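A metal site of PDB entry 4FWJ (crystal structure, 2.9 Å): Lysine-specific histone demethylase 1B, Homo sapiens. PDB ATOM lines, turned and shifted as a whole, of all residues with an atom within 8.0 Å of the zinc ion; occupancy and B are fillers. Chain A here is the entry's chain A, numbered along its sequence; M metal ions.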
ATOM      1  N   GLN A 115     -22.564 -26.071 -28.130  1.00  0.00           N
ATOM      2  CA  GLN A 115     -21.277 -26.603 -28.524  1.00  0.00           C
ATOM      3  C   GLN A 115     -20.256 -26.202 -27.504  1.00  0.00           C
ATOM      4  O   GLN A 115     -20.376 -25.161 -26.850  1.00  0.00           O
ATOM      5  CB  GLN A 115     -20.829 -26.046 -29.863  1.00  0.00           C
ATOM      6  CG  GLN A 115     -21.821 -26.208 -30.992  1.00  0.00           C
ATOM      7  CD  GLN A 115     -21.768 -25.026 -31.921  1.00  0.00           C
ATOM      8  OE1 GLN A 115     -21.334 -25.135 -33.064  1.00  0.00           O
ATOM      9  NE2 GLN A 115     -22.179 -23.858 -31.412  1.00  0.00           N
ATOM     10  N   CYS A 116     -19.220 -27.022 -27.396  1.00  0.00           N
ATOM     11  CA  CYS A 116     -18.074 -26.701 -26.593  1.00  0.00           C
ATOM     12  C   CYS A 116     -17.398 -25.489 -27.202  1.00  0.00           C
ATOM     13  O   CYS A 116     -17.256 -25.401 -28.426  1.00  0.00           O
ATOM     14  CB  CYS A 116     -17.130 -27.887 -26.581  1.00  0.00           C
ATOM     15  SG  CYS A 116     -15.752 -27.731 -25.427  1.00  0.00           S
ATOM     16  N   THR A 117     -16.980 -24.554 -26.364  1.00  0.00           N
ATOM     17  CA  THR A 117     -16.291 -23.358 -26.856  1.00  0.00           C
ATOM     18  C   THR A 117     -14.781 -23.516 -26.984  1.00  0.00           C
ATOM     19  O   THR A 117     -14.132 -22.665 -27.592  1.00  0.00           O
ATOM     20  CB  THR A 117     -16.587 -22.119 -26.008  1.00  0.00           C
ATOM     21  OG1 THR A 117     -16.164 -22.363 -24.655  1.00  0.00           O
ATOM     22  CG2 THR A 117     -18.068 -21.805 -26.055  1.00  0.00           C
ATOM     23  N   LYS A 118     -14.214 -24.562 -26.386  1.00  0.00           N
ATOM     24  CA  LYS A 118     -12.812 -24.896 -26.618  1.00  0.00           C
ATOM     25  C   LYS A 118     -12.678 -25.085 -28.130  1.00  0.00           C
ATOM     26  O   LYS A 118     -13.370 -25.915 -28.721  1.00  0.00           O
ATOM     27  CB  LYS A 118     -12.410 -26.165 -25.853  1.00  0.00           C
ATOM     28  CG  LYS A 118     -10.912 -26.408 -25.755  1.00  0.00           C
ATOM     29  CD  LYS A 118     -10.562 -27.883 -25.574  1.00  0.00           C
ATOM     30  CE  LYS A 118     -10.678 -28.355 -24.127  1.00  0.00           C
ATOM     31  NZ  LYS A 118     -10.437 -29.824 -23.974  1.00  0.00           N
ATOM     32  N   PRO A 119     -11.810 -24.277 -28.780  1.00  0.00           N
ATOM     33  CA  PRO A 119     -11.797 -24.190 -30.251  1.00  0.00           C
ATOM     34  C   PRO A 119     -11.453 -25.504 -30.933  1.00  0.00           C
ATOM     35  O   PRO A 119     -11.995 -25.808 -31.997  1.00  0.00           O
ATOM     36  CB  PRO A 119     -10.706 -23.145 -30.524  1.00  0.00           C
ATOM     37  CG  PRO A 119      -9.811 -23.215 -29.328  1.00  0.00           C
ATOM     38  CD  PRO A 119     -10.751 -23.454 -28.174  1.00  0.00           C
ATOM     39  N   GLU A 120     -10.551 -26.277 -30.325  1.00  0.00           N
ATOM     40  CA  GLU A 120     -10.088 -27.554 -30.886  1.00  0.00           C
ATOM     41  C   GLU A 120     -11.166 -28.644 -30.827  1.00  0.00           C
ATOM     42  O   GLU A 120     -11.104 -29.628 -31.553  1.00  0.00           O
ATOM     43  CB  GLU A 120      -8.808 -28.011 -30.172  1.00  0.00           C
ATOM     44  N   CYS A 121     -12.157 -28.451 -29.965  1.00  0.00           N
ATOM     45  CA  CYS A 121     -13.164 -29.472 -29.686  1.00  0.00           C
ATOM     46  C   CYS A 121     -14.494 -29.248 -30.433  1.00  0.00           C
ATOM     47  O   CYS A 121     -14.860 -30.032 -31.303  1.00  0.00           O
ATOM     48  CB  CYS A 121     -13.395 -29.567 -28.173  1.00  0.00           C
ATOM     49  SG  CYS A 121     -14.841 -30.531 -27.712  1.00  0.00           S
ATOM     50  N   ARG A 122     -15.204 -28.194 -30.029  1.00  0.00           N
ATOM     51  CA  ARG A 122     -16.441 -27.734 -30.669  1.00  0.00           C
ATOM     52  C   ARG A 122     -17.622 -28.727 -30.636  1.00  0.00           C
ATOM     53  O   ARG A 122     -18.588 -28.540 -31.381  1.00  0.00           O
ATOM     54  CB  ARG A 122     -16.154 -27.265 -32.103  1.00  0.00           C
ATOM     55  CG  ARG A 122     -15.276 -26.013 -32.200  1.00  0.00           C
ATOM     56  CD  ARG A 122     -16.069 -24.782 -32.661  1.00  0.00           C
ATOM     57  NE  ARG A 122     -16.947 -24.241 -31.627  1.00  0.00           N
ATOM     58  CZ  ARG A 122     -17.900 -23.319 -31.829  1.00  0.00           C
ATOM     59  NH1 ARG A 122     -18.104 -22.834 -33.061  1.00  0.00           N
ATOM     60  NH2 ARG A 122     -18.640 -22.894 -30.819  1.00  0.00           N
ATOM     61  N   LYS A 123     -17.562 -29.757 -29.777  1.00  0.00           N
ATOM     62  CA  LYS A 123     -18.605 -30.815 -29.702  1.00  0.00           C
ATOM     63  C   LYS A 123     -19.966 -30.352 -29.165  1.00  0.00           C
ATOM     64  O   LYS A 123     -20.035 -29.504 -28.266  1.00  0.00           O
ATOM     65  CB  LYS A 123     -18.133 -31.979 -28.839  1.00  0.00           C
ATOM     66  CG  LYS A 123     -17.598 -33.177 -29.588  1.00  0.00           C
ATOM     67  CD  LYS A 123     -16.085 -33.230 -29.516  1.00  0.00           C
ATOM     68  CE  LYS A 123     -15.559 -34.617 -29.773  1.00  0.00           C
ATOM     69  NZ  LYS A 123     -15.487 -35.397 -28.512  1.00  0.00           N
ATOM     70  N   TRP A 124     -21.045 -30.935 -29.705  1.00  0.00           N
ATOM     71  CA  TRP A 124     -22.412 -30.645 -29.280  1.00  0.00           C
ATOM     72  C   TRP A 124     -22.806 -31.454 -28.081  1.00  0.00           C
ATOM     73  O   TRP A 124     -22.655 -32.680 -28.093  1.00  0.00           O
ATOM     74  CB  TRP A 124     -23.380 -30.976 -30.397  1.00  0.00           C
ATOM     75  CG  TRP A 124     -23.542 -29.885 -31.425  1.00  0.00           C
ATOM     76  CD1 TRP A 124     -23.073 -29.866 -32.729  1.00  0.00           C
ATOM     77  CD2 TRP A 124     -24.268 -28.617 -31.272  1.00  0.00           C
ATOM     78  NE1 TRP A 124     -23.430 -28.713 -33.363  1.00  0.00           N
ATOM     79  CE2 TRP A 124     -24.150 -27.920 -32.554  1.00  0.00           C
ATOM     80  CE3 TRP A 124     -24.982 -28.019 -30.239  1.00  0.00           C
ATOM     81  CZ2 TRP A 124     -24.725 -26.685 -32.771  1.00  0.00           C
ATOM     82  CZ3 TRP A 124     -25.554 -26.764 -30.466  1.00  0.00           C
ATOM     83  CH2 TRP A 124     -25.433 -26.117 -31.702  1.00  0.00           C
ATOM     84  N   ARG A 125     -23.326 -30.799 -27.047  1.00  0.00           N
ATOM     85  CA  ARG A 125     -23.773 -31.479 -25.817  1.00  0.00           C
ATOM     86  C   ARG A 125     -25.207 -31.092 -25.402  1.00  0.00           C
ATOM     87  O   ARG A 125     -25.682 -30.016 -25.749  1.00  0.00           O
ATOM     88  CB  ARG A 125     -22.798 -31.197 -24.664  1.00  0.00           C
ATOM     89  CG  ARG A 125     -21.685 -32.233 -24.508  1.00  0.00           C
ATOM     90  CD  ARG A 125     -20.750 -32.265 -25.695  1.00  0.00           C
ATOM     91  NE  ARG A 125     -19.447 -32.902 -25.442  1.00  0.00           N
ATOM     92  CZ  ARG A 125     -19.133 -34.168 -25.731  1.00  0.00           C
ATOM     93  NH1 ARG A 125     -20.020 -34.994 -26.279  1.00  0.00           N
ATOM     94  NH2 ARG A 125     -17.909 -34.598 -25.472  1.00  0.00           N
ATOM     95  N   TYR A 141     -19.431 -22.094 -22.453  1.00  0.00           N
ATOM     96  CA  TYR A 141     -19.584 -23.535 -22.164  1.00  0.00           C
ATOM     97  C   TYR A 141     -18.439 -24.424 -22.643  1.00  0.00           C
ATOM     98  O   TYR A 141     -17.859 -24.186 -23.710  1.00  0.00           O
ATOM     99  CB  TYR A 141     -20.912 -24.067 -22.719  1.00  0.00           C
ATOM    100  CG  TYR A 141     -21.067 -25.559 -22.518  1.00  0.00           C
ATOM    101  CD1 TYR A 141     -21.566 -26.071 -21.314  1.00  0.00           C
ATOM    102  CD2 TYR A 141     -20.703 -26.459 -23.524  1.00  0.00           C
ATOM    103  CE1 TYR A 141     -21.721 -27.434 -21.125  1.00  0.00           C
ATOM    104  CE2 TYR A 141     -20.832 -27.831 -23.344  1.00  0.00           C
ATOM    105  CZ  TYR A 141     -21.345 -28.313 -22.136  1.00  0.00           C
ATOM    106  OH  TYR A 141     -21.478 -29.665 -21.948  1.00  0.00           O
ATOM    107  N   ARG A 142     -18.153 -25.457 -21.845  1.00  0.00           N
ATOM    108  CA  ARG A 142     -17.202 -26.520 -22.171  1.00  0.00           C
ATOM    109  C   ARG A 142     -17.716 -27.901 -21.751  1.00  0.00           C
ATOM    110  O   ARG A 142     -18.474 -28.017 -20.790  1.00  0.00           O
ATOM    111  CB  ARG A 142     -15.865 -26.245 -21.489  1.00  0.00           C
ATOM    112  CG  ARG A 142     -15.146 -25.008 -21.979  1.00  0.00           C
ATOM    113  CD  ARG A 142     -13.769 -24.914 -21.365  1.00  0.00           C
ATOM    114  NE  ARG A 142     -12.774 -24.600 -22.383  1.00  0.00           N
ATOM    115  CZ  ARG A 142     -11.556 -24.129 -22.132  1.00  0.00           C
ATOM    116  NH1 ARG A 142     -11.163 -23.896 -20.883  1.00  0.00           N
ATOM    117  NH2 ARG A 142     -10.733 -23.881 -23.152  1.00  0.00           N
ATOM    118  N   CYS A 143     -17.290 -28.942 -22.474  1.00  0.00           N
ATOM    119  CA  CYS A 143     -17.664 -30.320 -22.143  1.00  0.00           C
ATOM    120  C   CYS A 143     -17.401 -30.617 -20.676  1.00  0.00           C
ATOM    121  O   CYS A 143     -16.265 -30.525 -20.208  1.00  0.00           O
ATOM    122  CB  CYS A 143     -16.889 -31.311 -23.003  1.00  0.00           C
ATOM    123  SG  CYS A 143     -17.149 -31.121 -24.776  1.00  0.00           S
ATOM    124  N   GLY A 144     -18.467 -30.951 -19.955  1.00  0.00           N
ATOM    125  CA  GLY A 144     -18.338 -31.315 -18.550  1.00  0.00           C
ATOM    126  C   GLY A 144     -19.264 -30.528 -17.627  1.00  0.00           C
ATOM    127  O   GLY A 144     -20.235 -31.092 -17.114  1.00  0.00           O
ATOM    128  N   SER A 156      -9.985 -31.723 -18.788  1.00  0.00           N
ATOM    129  CA  SER A 156     -10.238 -31.554 -20.238  1.00  0.00           C
ATOM    130  C   SER A 156     -10.397 -32.898 -20.976  1.00  0.00           C
ATOM    131  O   SER A 156     -10.057 -33.042 -22.151  1.00  0.00           O
ATOM    132  CB  SER A 156      -9.162 -30.679 -20.892  1.00  0.00           C
ATOM    133  N   ASP A 157     -10.933 -33.882 -20.238  1.00  0.00           N
ATOM    134  CA  ASP A 157     -11.124 -35.242 -20.737  1.00  0.00           C
ATOM    135  C   ASP A 157     -12.543 -35.446 -21.271  1.00  0.00           C
ATOM    136  O   ASP A 157     -12.768 -36.295 -22.130  1.00  0.00           O
ATOM    137  CB  ASP A 157     -10.797 -36.266 -19.645  1.00  0.00           C
ATOM    138  N   HIS A 158     -13.505 -34.660 -20.772  1.00  0.00           N
ATOM    139  CA  HIS A 158     -14.893 -34.712 -21.247  1.00  0.00           C
ATOM    140  C   HIS A 158     -15.015 -34.328 -22.694  1.00  0.00           C
ATOM    141  O   HIS A 158     -15.986 -34.679 -23.349  1.00  0.00           O
ATOM    142  CB  HIS A 158     -15.782 -33.795 -20.418  1.00  0.00           C
ATOM    143  CG  HIS A 158     -15.844 -34.155 -18.958  1.00  0.00           C
ATOM    144  ND1 HIS A 158     -14.842 -33.858 -18.100  1.00  0.00           N
ATOM    145  CD2 HIS A 158     -16.832 -34.775 -18.210  1.00  0.00           C
ATOM    146  CE1 HIS A 158     -15.169 -34.283 -16.872  1.00  0.00           C
ATOM    147  NE2 HIS A 158     -16.391 -34.840 -16.938  1.00  0.00           N
ATOM    148  N   CYS A 159     -14.024 -33.582 -23.198  1.00  0.00           N
ATOM    149  CA  CYS A 159     -13.988 -33.192 -24.605  1.00  0.00           C
ATOM    150  C   CYS A 159     -13.645 -34.342 -25.542  1.00  0.00           C
ATOM    151  O   CYS A 159     -13.653 -34.179 -26.758  1.00  0.00           O
ATOM    152  CB  CYS A 159     -12.984 -32.059 -24.819  1.00  0.00           C
ATOM    153  SG  CYS A 159     -13.607 -30.459 -24.301  1.00  0.00           S
ATOM    154  N   SER A 160     -13.348 -35.499 -24.968  1.00  0.00           N
ATOM    155  CA  SER A 160     -12.998 -36.675 -25.748  1.00  0.00           C
ATOM    156  C   SER A 160     -14.210 -37.545 -25.972  1.00  0.00           C
ATOM    157  O   SER A 160     -14.218 -38.357 -26.897  1.00  0.00           O
ATOM    158  CB  SER A 160     -11.891 -37.479 -25.056  1.00  0.00           C
ATOM    159  OG  SER A 160     -10.621 -37.154 -25.595  1.00  0.00           O
ATOM    160  N   LEU A 161     -15.228 -37.394 -25.144  1.00  0.00           N
ATOM    161  CA  LEU A 161     -16.394 -38.280 -25.248  1.00  0.00           C
ATOM    162  C   LEU A 161     -17.154 -38.097 -26.558  1.00  0.00           C
ATOM    163  O   LEU A 161     -17.339 -36.973 -27.013  1.00  0.00           O
ATOM    164  CB  LEU A 161     -17.302 -38.096 -24.016  1.00  0.00           C
ATOM    165  CG  LEU A 161     -16.757 -38.657 -22.704  1.00  0.00           C
ATOM    166  CD1 LEU A 161     -17.703 -38.355 -21.545  1.00  0.00           C
ATOM    167  CD2 LEU A 161     -16.541 -40.163 -22.827  1.00  0.00           C
HETATM  168 ZN    ZN M   1     -15.370 -30.132 -25.579  1.00  0.00          ZN
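The side-chain sulfur (SG) of Cys 143 lies close to the guanidinium group (NE) of Arg 125 (3.0 Å). O of Cys 159 is in hydrogen-bond range of NZ of Lys 123 (2.8 Å). SG of Cys 159 sits close to NZ of Lys 118, at 3.2 Å. The backbone NH (N) of Lys 123 lies close to the side-chain sulfur (SG) of Cys 121. The backbone NH of Cys 116 is in hydrogen-bond range of the backbone carbonyl oxygen of Lys 123 (2.8 Å). The backbone carbonyl oxygen (O) of Cys 116 sits close to the guanidinium group (NE) of Arg 122 (3.4 Å). The side-chain sulfur of Cys 116 lies close to the backbone NH of Lys 118, at 3.7 Å.
Four residues have an atom within 4 Å of the zinc ion: Cys 116, Cys 121, Cys 143 and Cys 159.
The zinc ion is bound by the side-chain sulfur of Cys 143 (2.2 Å), the side-chain sulfur of Cys 159 (2.2 Å), the side-chain sulfur of Cys 121 (2.2 Å) and the side-chain sulfur of Cys 116 (2.4 Å). The zinc ion has four donor atoms within binding distance.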
